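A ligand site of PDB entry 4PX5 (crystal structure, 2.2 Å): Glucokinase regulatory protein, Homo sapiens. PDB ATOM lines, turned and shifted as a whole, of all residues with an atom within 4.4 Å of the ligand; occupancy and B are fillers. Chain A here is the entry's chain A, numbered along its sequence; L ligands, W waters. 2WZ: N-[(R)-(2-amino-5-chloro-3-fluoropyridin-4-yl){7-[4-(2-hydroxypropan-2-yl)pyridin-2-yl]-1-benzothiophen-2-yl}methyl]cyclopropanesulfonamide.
Water W1 lies within hydrogen-bond range of an oxygen (O1) of the ligand (2.5 Å), the side-chain hydroxyl of Tyr 36 (2.7 Å) and the backbone carbonyl oxygen of Ala 533 (2.8 Å).
Water W2 bridges the side-chain carboxylate (OE2) of Glu 44 (2.7 Å) and a nitrogen (N2) of the ligand (3.1 Å).
O of Gly 193 sits at hydrogen-bond distance from N4 of the ligand, at 2.9 Å.
The indole nitrogen of Trp 529 sits close to an oxygen (O3) of the ligand (3.3 Å).
An oxygen (O2) of the ligand lies within hydrogen-bond range of the backbone NH (N) of Asp 229.
A nitrogen (N4) of the ligand is in hydrogen-bond range of the backbone carbonyl oxygen (O) of Met 225 (3.1 Å).
An oxygen (O1) of the ligand sits at hydrogen-bond distance from the guanidinium group (NH2) of Arg 537 (3.1 Å).
The guanidinium group (NE) of Arg 227 lies within hydrogen-bond range of an oxygen (O3) of the ligand, 3.3 Å away.
The backbone NH of Asn 228 sits at hydrogen-bond distance from an oxygen (O2) of the ligand (3.3 Å).
O of Gly 193 is in hydrogen-bond range of ND2 of Asn 221.
The indole nitrogen of Trp 529 sits at hydrogen-bond distance from the side-chain carboxylate of Asp 229 (2.9 Å).
OD2 of Asp 229 lies within salt-bridge range of NH2 of Arg 227 (2.7 Å).
NH1 of Arg 227 lies within hydrogen-bond range of OG of Ser 195 (3.0 Å).
The backbone NH (N) of Arg 227 lies within hydrogen-bond range of the backbone carbonyl oxygen (O) of Leu 194, at 3.1 Å.
The side-chain carboxylate (OE2) of Glu 44 is in salt-bridge range of the guanidinium group (NH2) of Arg 530 (2.6 Å).
CE1 of His 21 touches C24 of the ligand (3.3 Å).
Tyr 36 touches the ligand.
Val 40 touches the ligand.
Pro 41 touches the ligand (CG to F1, 3.4 Å).
Glu 44 touches the ligand (OE1 to C16, 3.5 Å).
Ser 195 touches the ligand.
Asn 221 touches the ligand.
His 516 touches the ligand.
Lys 526 touches the ligand.
CB of Ala 533 touches N3 of the ligand, 3.6 Å away.
Hydrophobic or aromatic side chains within 4 Å of the ligand: His 21, Tyr 36, Val 40, Pro 41, His 516, Trp 529 and Ala 533.
Of the 24 residues printed, 17 come within 4 Å of the ligand.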
ATOM      1  N   HIS A  21      14.402   5.178 -27.251  1.00  0.00           N
ATOM      2  CA  HIS A  21      14.094   5.299 -25.837  1.00  0.00           C
ATOM      3  C   HIS A  21      13.618   3.999 -25.225  1.00  0.00           C
ATOM      4  O   HIS A  21      13.368   3.941 -24.023  1.00  0.00           O
ATOM      5  CB  HIS A  21      13.078   6.423 -25.613  1.00  0.00           C
ATOM      6  CG  HIS A  21      11.837   6.257 -26.408  1.00  0.00           C
ATOM      7  ND1 HIS A  21      10.585   6.364 -25.856  1.00  0.00           N
ATOM      8  CD2 HIS A  21      11.645   5.938 -27.717  1.00  0.00           C
ATOM      9  CE1 HIS A  21       9.679   6.159 -26.782  1.00  0.00           C
ATOM     10  NE2 HIS A  21      10.294   5.888 -27.916  1.00  0.00           N
ATOM     11  N   ILE A  23      14.268   0.719 -23.405  1.00  0.00           N
ATOM     12  CA  ILE A  23      15.403   0.185 -22.685  1.00  0.00           C
ATOM     13  C   ILE A  23      15.750  -1.197 -23.233  1.00  0.00           C
ATOM     14  O   ILE A  23      14.852  -2.028 -23.489  1.00  0.00           O
ATOM     15  CB  ILE A  23      15.169  -0.022 -21.197  1.00  0.00           C
ATOM     16  CG1 ILE A  23      14.445   1.177 -20.513  1.00  0.00           C
ATOM     17  CG2 ILE A  23      16.474  -0.379 -20.481  1.00  0.00           C
ATOM     18  CD1 ILE A  23      14.979   2.538 -20.772  1.00  0.00           C
ATOM     19  N   TYR A  36      17.072  -2.249 -14.717  1.00  0.00           N
ATOM     20  CA  TYR A  36      15.906  -2.361 -15.596  1.00  0.00           C
ATOM     21  C   TYR A  36      14.610  -2.391 -14.756  1.00  0.00           C
ATOM     22  O   TYR A  36      13.691  -1.593 -15.004  1.00  0.00           O
ATOM     23  CB  TYR A  36      16.030  -3.536 -16.559  1.00  0.00           C
ATOM     24  CG  TYR A  36      14.921  -3.611 -17.612  1.00  0.00           C
ATOM     25  CD1 TYR A  36      13.652  -4.071 -17.283  1.00  0.00           C
ATOM     26  CD2 TYR A  36      15.129  -3.208 -18.885  1.00  0.00           C
ATOM     27  CE1 TYR A  36      12.643  -4.123 -18.218  1.00  0.00           C
ATOM     28  CE2 TYR A  36      14.135  -3.302 -19.814  1.00  0.00           C
ATOM     29  CZ  TYR A  36      12.882  -3.764 -19.469  1.00  0.00           C
ATOM     30  OH  TYR A  36      11.852  -3.834 -20.413  1.00  0.00           O
ATOM     31  N   ALA A  39      13.355   0.845 -13.611  1.00  0.00           N
ATOM     32  CA  ALA A  39      12.764   1.648 -14.647  1.00  0.00           C
ATOM     33  C   ALA A  39      11.336   1.242 -15.093  1.00  0.00           C
ATOM     34  O   ALA A  39      10.665   2.020 -15.710  1.00  0.00           O
ATOM     35  CB  ALA A  39      13.688   1.640 -15.853  1.00  0.00           C
ATOM     36  N   VAL A  40      10.887   0.012 -14.799  1.00  0.00           N
ATOM     37  CA  VAL A  40       9.533  -0.390 -15.165  1.00  0.00           C
ATOM     38  C   VAL A  40       8.554   0.514 -14.404  1.00  0.00           C
ATOM     39  O   VAL A  40       8.601   0.599 -13.198  1.00  0.00           O
ATOM     40  CB  VAL A  40       9.253  -1.845 -14.790  1.00  0.00           C
ATOM     41  CG1 VAL A  40       7.891  -2.324 -15.359  1.00  0.00           C
ATOM     42  CG2 VAL A  40      10.381  -2.728 -15.285  1.00  0.00           C
ATOM     43  N   PRO A  41       7.663   1.196 -15.120  1.00  0.00           N
ATOM     44  CA  PRO A  41       6.631   1.960 -14.406  1.00  0.00           C
ATOM     45  C   PRO A  41       5.834   1.099 -13.458  1.00  0.00           C
ATOM     46  O   PRO A  41       5.528  -0.075 -13.780  1.00  0.00           O
ATOM     47  CB  PRO A  41       5.762   2.499 -15.546  1.00  0.00           C
ATOM     48  CG  PRO A  41       6.726   2.641 -16.665  1.00  0.00           C
ATOM     49  CD  PRO A  41       7.666   1.497 -16.564  1.00  0.00           C
ATOM     50  N   GLU A  44       3.094  -0.779 -14.874  1.00  0.00           N
ATOM     51  CA  GLU A  44       3.315  -1.822 -15.828  1.00  0.00           C
ATOM     52  C   GLU A  44       3.976  -3.043 -15.190  1.00  0.00           C
ATOM     53  O   GLU A  44       4.148  -4.077 -15.852  1.00  0.00           O
ATOM     54  CB  GLU A  44       4.240  -1.250 -16.921  1.00  0.00           C
ATOM     55  CG  GLU A  44       3.534  -0.183 -17.743  1.00  0.00           C
ATOM     56  CD  GLU A  44       2.355  -0.728 -18.592  1.00  0.00           C
ATOM     57  OE1 GLU A  44       2.406  -1.856 -19.091  1.00  0.00           O
ATOM     58  OE2 GLU A  44       1.392   0.022 -18.794  1.00  0.00           O
ATOM     59  N   SER A  46       5.060  -6.391 -13.116  1.00  0.00           N
ATOM     60  CA  SER A  46       4.637  -7.680 -12.611  1.00  0.00           C
ATOM     61  C   SER A  46       4.477  -7.658 -11.076  1.00  0.00           C
ATOM     62  O   SER A  46       5.435  -7.341 -10.401  1.00  0.00           O
ATOM     63  CB  SER A  46       5.717  -8.695 -12.987  1.00  0.00           C
ATOM     64  OG  SER A  46       5.327  -9.978 -12.602  1.00  0.00           O
ATOM     65  N   GLY A 193      -1.411   5.613 -15.655  1.00  0.00           N
ATOM     66  CA  GLY A 193      -0.036   5.403 -16.017  1.00  0.00           C
ATOM     67  C   GLY A 193       0.744   6.658 -16.231  1.00  0.00           C
ATOM     68  O   GLY A 193       1.939   6.587 -16.529  1.00  0.00           O
ATOM     69  N   LEU A 194       0.077   7.796 -16.113  1.00  0.00           N
ATOM     70  CA  LEU A 194       0.634   9.089 -16.522  1.00  0.00           C
ATOM     71  C   LEU A 194       1.114   8.929 -17.980  1.00  0.00           C
ATOM     72  O   LEU A 194       2.314   9.175 -18.328  1.00  0.00           O
ATOM     73  CB  LEU A 194       1.745   9.559 -15.608  1.00  0.00           C
ATOM     74  CG  LEU A 194       1.392   9.923 -14.154  1.00  0.00           C
ATOM     75  CD1 LEU A 194       2.492  10.769 -13.529  1.00  0.00           C
ATOM     76  CD2 LEU A 194       0.111  10.692 -14.080  1.00  0.00           C
ATOM     77  N   SER A 195       0.156   8.523 -18.800  1.00  0.00           N
ATOM     78  CA  SER A 195       0.423   7.983 -20.072  1.00  0.00           C
ATOM     79  C   SER A 195      -0.389   8.539 -21.242  1.00  0.00           C
ATOM     80  O   SER A 195       0.173   8.638 -22.302  1.00  0.00           O
ATOM     81  CB  SER A 195       0.128   6.474 -20.004  1.00  0.00           C
ATOM     82  OG  SER A 195      -0.245   6.016 -21.247  1.00  0.00           O
ATOM     83  N   ASN A 221       1.912   6.745 -10.974  1.00  0.00           N
ATOM     84  CA  ASN A 221       3.361   6.584 -11.087  1.00  0.00           C
ATOM     85  C   ASN A 221       4.053   7.808 -10.581  1.00  0.00           C
ATOM     86  O   ASN A 221       3.504   8.856 -10.604  1.00  0.00           O
ATOM     87  CB  ASN A 221       3.794   6.402 -12.507  1.00  0.00           C
ATOM     88  CG  ASN A 221       3.556   5.013 -13.013  1.00  0.00           C
ATOM     89  OD1 ASN A 221       3.790   3.989 -12.317  1.00  0.00           O
ATOM     90  ND2 ASN A 221       3.072   4.945 -14.229  1.00  0.00           N
ATOM     91  N   MET A 225       8.611   8.231 -13.700  1.00  0.00           N
ATOM     92  CA  MET A 225       8.156   7.141 -14.548  1.00  0.00           C
ATOM     93  C   MET A 225       7.052   7.479 -15.543  1.00  0.00           C
ATOM     94  O   MET A 225       6.554   6.589 -16.237  1.00  0.00           O
ATOM     95  CB  MET A 225       7.658   6.018 -13.659  1.00  0.00           C
ATOM     96  CG  MET A 225       8.794   5.311 -12.979  1.00  0.00           C
ATOM     97  SD  MET A 225       8.110   4.273 -11.678  1.00  0.00           S
ATOM     98  CE  MET A 225       9.491   3.250 -11.245  1.00  0.00           C
ATOM     99  N   ALA A 226       6.656   8.734 -15.618  1.00  0.00           N
ATOM    100  CA  ALA A 226       5.673   9.105 -16.621  1.00  0.00           C
ATOM    101  C   ALA A 226       6.223   8.791 -17.986  1.00  0.00           C
ATOM    102  O   ALA A 226       7.471   8.811 -18.176  1.00  0.00           O
ATOM    103  CB  ALA A 226       5.385  10.591 -16.518  1.00  0.00           C
ATOM    104  N   ARG A 227       5.307   8.538 -18.927  1.00  0.00           N
ATOM    105  CA  ARG A 227       5.670   8.251 -20.261  1.00  0.00           C
ATOM    106  C   ARG A 227       6.448   9.343 -20.916  1.00  0.00           C
ATOM    107  O   ARG A 227       6.040  10.522 -20.918  1.00  0.00           O
ATOM    108  CB  ARG A 227       4.460   8.016 -21.153  1.00  0.00           C
ATOM    109  CG  ARG A 227       4.246   6.587 -21.511  1.00  0.00           C
ATOM    110  CD  ARG A 227       2.943   6.360 -22.191  1.00  0.00           C
ATOM    111  NE  ARG A 227       3.153   6.115 -23.581  1.00  0.00           N
ATOM    112  CZ  ARG A 227       2.192   5.822 -24.444  1.00  0.00           C
ATOM    113  NH1 ARG A 227       0.926   5.770 -24.044  1.00  0.00           N
ATOM    114  NH2 ARG A 227       2.527   5.567 -25.706  1.00  0.00           N
ATOM    115  N   ASN A 228       7.490   8.919 -21.620  1.00  0.00           N
ATOM    116  CA  ASN A 228       8.321   9.805 -22.318  1.00  0.00           C
ATOM    117  C   ASN A 228       8.298   9.504 -23.790  1.00  0.00           C
ATOM    118  O   ASN A 228       9.341   9.633 -24.373  1.00  0.00           O
ATOM    119  CB  ASN A 228       9.756   9.663 -21.759  1.00  0.00           C
ATOM    120  CG  ASN A 228      10.595  10.915 -21.943  1.00  0.00           C
ATOM    121  OD1 ASN A 228      10.100  12.060 -21.998  1.00  0.00           O
ATOM    122  ND2 ASN A 228      11.888  10.716 -22.054  1.00  0.00           N
ATOM    123  N   ASP A 229       7.195   9.069 -24.409  1.00  0.00           N
ATOM    124  CA  ASP A 229       7.265   8.821 -25.837  1.00  0.00           C
ATOM    125  C   ASP A 229       6.719   9.967 -26.642  1.00  0.00           C
ATOM    126  O   ASP A 229       5.841  10.735 -26.194  1.00  0.00           O
ATOM    127  CB  ASP A 229       6.720   7.417 -26.335  1.00  0.00           C
ATOM    128  CG  ASP A 229       5.253   7.333 -26.368  1.00  0.00           C
ATOM    129  OD1 ASP A 229       4.708   8.089 -25.568  1.00  0.00           O
ATOM    130  OD2 ASP A 229       4.630   6.519 -27.164  1.00  0.00           O
ATOM    131  N   HIS A 516       0.723 -11.915 -16.847  1.00  0.00           N
ATOM    132  CA  HIS A 516       0.627 -11.049 -18.050  1.00  0.00           C
ATOM    133  C   HIS A 516      -0.460 -11.505 -19.000  1.00  0.00           C
ATOM    134  O   HIS A 516      -0.697 -12.694 -19.145  1.00  0.00           O
ATOM    135  CB  HIS A 516       1.954 -11.086 -18.793  1.00  0.00           C
ATOM    136  CG  HIS A 516       3.118 -10.591 -17.991  1.00  0.00           C
ATOM    137  ND1 HIS A 516       3.283  -9.275 -17.658  1.00  0.00           N
ATOM    138  CD2 HIS A 516       4.193 -11.247 -17.492  1.00  0.00           C
ATOM    139  CE1 HIS A 516       4.396  -9.134 -16.956  1.00  0.00           C
ATOM    140  NE2 HIS A 516       4.984 -10.304 -16.880  1.00  0.00           N
ATOM    141  N   LYS A 526       0.400   2.746 -26.315  1.00  0.00           N
ATOM    142  CA  LYS A 526       0.726   2.088 -25.041  1.00  0.00           C
ATOM    143  C   LYS A 526       0.778   0.558 -25.149  1.00  0.00           C
ATOM    144  O   LYS A 526       1.699  -0.117 -24.665  1.00  0.00           O
ATOM    145  CB  LYS A 526      -0.304   2.455 -23.950  1.00  0.00           C
ATOM    146  CG  LYS A 526       0.029   1.837 -22.611  1.00  0.00           C
ATOM    147  CD  LYS A 526      -0.827   2.406 -21.488  1.00  0.00           C
ATOM    148  CE  LYS A 526      -2.315   2.054 -21.637  1.00  0.00           C
ATOM    149  NZ  LYS A 526      -2.948   2.783 -20.539  1.00  0.00           N
ATOM    150  N   TRP A 529       3.767  -0.756 -26.982  1.00  0.00           N
ATOM    151  CA  TRP A 529       4.993  -0.778 -26.124  1.00  0.00           C
ATOM    152  C   TRP A 529       4.950  -1.888 -25.116  1.00  0.00           C
ATOM    153  O   TRP A 529       5.973  -2.497 -24.813  1.00  0.00           O
ATOM    154  CB  TRP A 529       5.200   0.553 -25.416  1.00  0.00           C
ATOM    155  CG  TRP A 529       5.443   1.712 -26.312  1.00  0.00           C
ATOM    156  CD1 TRP A 529       4.770   2.903 -26.321  1.00  0.00           C
ATOM    157  CD2 TRP A 529       6.479   1.835 -27.300  1.00  0.00           C
ATOM    158  NE1 TRP A 529       5.328   3.756 -27.249  1.00  0.00           N
ATOM    159  CE2 TRP A 529       6.356   3.116 -27.883  1.00  0.00           C
ATOM    160  CE3 TRP A 529       7.482   0.967 -27.764  1.00  0.00           C
ATOM    161  CZ2 TRP A 529       7.202   3.560 -28.890  1.00  0.00           C
ATOM    162  CZ3 TRP A 529       8.318   1.407 -28.811  1.00  0.00           C
ATOM    163  CH2 TRP A 529       8.161   2.706 -29.350  1.00  0.00           C
ATOM    164  N   ARG A 530       3.750  -2.208 -24.633  1.00  0.00           N
ATOM    165  CA  ARG A 530       3.600  -3.291 -23.642  1.00  0.00           C
ATOM    166  C   ARG A 530       3.848  -4.615 -24.389  1.00  0.00           C
ATOM    167  O   ARG A 530       4.517  -5.479 -23.871  1.00  0.00           O
ATOM    168  CB  ARG A 530       2.233  -3.251 -22.904  1.00  0.00           C
ATOM    169  CG  ARG A 530       1.979  -4.385 -21.861  1.00  0.00           C
ATOM    170  CD  ARG A 530       0.546  -4.262 -21.265  1.00  0.00           C
ATOM    171  NE  ARG A 530       0.397  -2.950 -20.662  1.00  0.00           N
ATOM    172  CZ  ARG A 530      -0.726  -2.253 -20.479  1.00  0.00           C
ATOM    173  NH1 ARG A 530      -1.864  -2.713 -20.859  1.00  0.00           N
ATOM    174  NH2 ARG A 530      -0.683  -1.040 -19.935  1.00  0.00           N
ATOM    175  N   ALA A 533       7.671  -4.871 -24.753  1.00  0.00           N
ATOM    176  CA  ALA A 533       8.283  -5.200 -23.489  1.00  0.00           C
ATOM    177  C   ALA A 533       8.002  -6.621 -23.067  1.00  0.00           C
ATOM    178  O   ALA A 533       8.892  -7.294 -22.513  1.00  0.00           O
ATOM    179  CB  ALA A 533       7.807  -4.266 -22.397  1.00  0.00           C
ATOM    180  N   MET A 534       6.757  -7.059 -23.234  1.00  0.00           N
ATOM    181  CA  MET A 534       6.454  -8.450 -22.971  1.00  0.00           C
ATOM    182  C   MET A 534       7.316  -9.410 -23.833  1.00  0.00           C
ATOM    183  O   MET A 534       7.732 -10.456 -23.339  1.00  0.00           O
ATOM    184  CB  MET A 534       4.989  -8.730 -23.186  1.00  0.00           C
ATOM    185  CG  MET A 534       4.144  -8.281 -22.021  1.00  0.00           C
ATOM    186  SD  MET A 534       2.464  -8.885 -22.168  1.00  0.00           S
ATOM    187  CE  MET A 534       1.975  -8.149 -23.721  1.00  0.00           C
ATOM    188  N   ARG A 537      10.678  -9.566 -22.284  1.00  0.00           N
ATOM    189  CA  ARG A 537      10.657 -10.249 -21.003  1.00  0.00           C
ATOM    190  C   ARG A 537      10.599 -11.781 -21.151  1.00  0.00           C
ATOM    191  O   ARG A 537      11.250 -12.501 -20.394  1.00  0.00           O
ATOM    192  CB  ARG A 537       9.505  -9.762 -20.119  1.00  0.00           C
ATOM    193  CG  ARG A 537       9.319 -10.524 -18.797  1.00  0.00           C
ATOM    194  CD  ARG A 537      10.384 -10.215 -17.735  1.00  0.00           C
ATOM    195  NE  ARG A 537      10.254  -8.842 -17.238  1.00  0.00           N
ATOM    196  CZ  ARG A 537      10.879  -8.311 -16.189  1.00  0.00           C
ATOM    197  NH1 ARG A 537      11.727  -8.998 -15.429  1.00  0.00           N
ATOM    198  NH2 ARG A 537      10.643  -7.037 -15.899  1.00  0.00           N
HETATM  199 CL1  2WZ L   1       3.797   1.696 -22.288  1.00  0.00          CL
HETATM  200  C4  2WZ L   1       3.963   2.802 -20.937  1.00  0.00           C
HETATM  201  C5  2WZ L   1       2.874   3.036 -20.087  1.00  0.00           C
HETATM  202  N2  2WZ L   1       2.972   3.845 -19.061  1.00  0.00           N
HETATM  203  C6  2WZ L   1       4.105   4.437 -18.763  1.00  0.00           C
HETATM  204  N4  2WZ L   1       4.196   5.267 -17.740  1.00  0.00           N
HETATM  205  C7  2WZ L   1       5.226   4.238 -19.547  1.00  0.00           C
HETATM  206  F1  2WZ L   1       6.358   4.905 -19.213  1.00  0.00           F
HETATM  207  C2  2WZ L   1       5.149   3.430 -20.651  1.00  0.00           C
HETATM  208  C1  2WZ L   1       6.395   3.181 -21.512  1.00  0.00           C
HETATM  209  N1  2WZ L   1       7.084   4.450 -21.847  1.00  0.00           N
HETATM  210  S2  2WZ L   1       7.275   4.803 -23.382  1.00  0.00           S
HETATM  211  O2  2WZ L   1       7.619   6.214 -23.500  1.00  0.00           O
HETATM  212  O3  2WZ L   1       5.982   4.595 -24.130  1.00  0.00           O
HETATM  213  C23 2WZ L   1       8.764   4.012 -23.966  1.00  0.00           C
HETATM  214  C24 2WZ L   1       8.379   3.544 -25.325  1.00  0.00           C
HETATM  215  C25 2WZ L   1       8.677   2.520 -24.204  1.00  0.00           C
HETATM  216  C3  2WZ L   1       7.286   2.162 -20.855  1.00  0.00           C
HETATM  217  C10 2WZ L   1       8.621   2.322 -20.568  1.00  0.00           C
HETATM  218  S1  2WZ L   1       6.778   0.570 -20.450  1.00  0.00           S
HETATM  219  C8  2WZ L   1       8.315   0.086 -19.928  1.00  0.00           C
HETATM  220  C9  2WZ L   1       9.209   1.173 -20.054  1.00  0.00           C
HETATM  221  C14 2WZ L   1      10.534   1.025 -19.603  1.00  0.00           C
HETATM  222  C13 2WZ L   1      10.948  -0.202 -19.123  1.00  0.00           C
HETATM  223  C12 2WZ L   1      10.052  -1.269 -19.059  1.00  0.00           C
HETATM  224  C11 2WZ L   1       8.726  -1.126 -19.474  1.00  0.00           C
HETATM  225  C15 2WZ L   1       7.797  -2.184 -19.398  1.00  0.00           C
HETATM  226  C19 2WZ L   1       8.108  -3.449 -18.848  1.00  0.00           C
HETATM  227  N3  2WZ L   1       6.585  -2.002 -19.911  1.00  0.00           N
HETATM  228  C16 2WZ L   1       5.663  -2.957 -19.834  1.00  0.00           C
HETATM  229  C17 2WZ L   1       5.882  -4.224 -19.299  1.00  0.00           C
HETATM  230  C18 2WZ L   1       7.156  -4.479 -18.827  1.00  0.00           C
HETATM  231  C20 2WZ L   1       7.489  -5.877 -18.260  1.00  0.00           C
HETATM  232  C21 2WZ L   1       7.077  -5.970 -16.826  1.00  0.00           C
HETATM  233  C22 2WZ L   1       6.773  -6.952 -19.107  1.00  0.00           C
HETATM  234  O1  2WZ L   1       8.886  -6.111 -18.305  1.00  0.00           O
HETATM  235  O   HOH W   1      10.309  -6.064 -20.393  1.00  0.00           O
HETATM  236  O   HOH W   2       0.858   2.300 -17.491  1.00  0.00           O
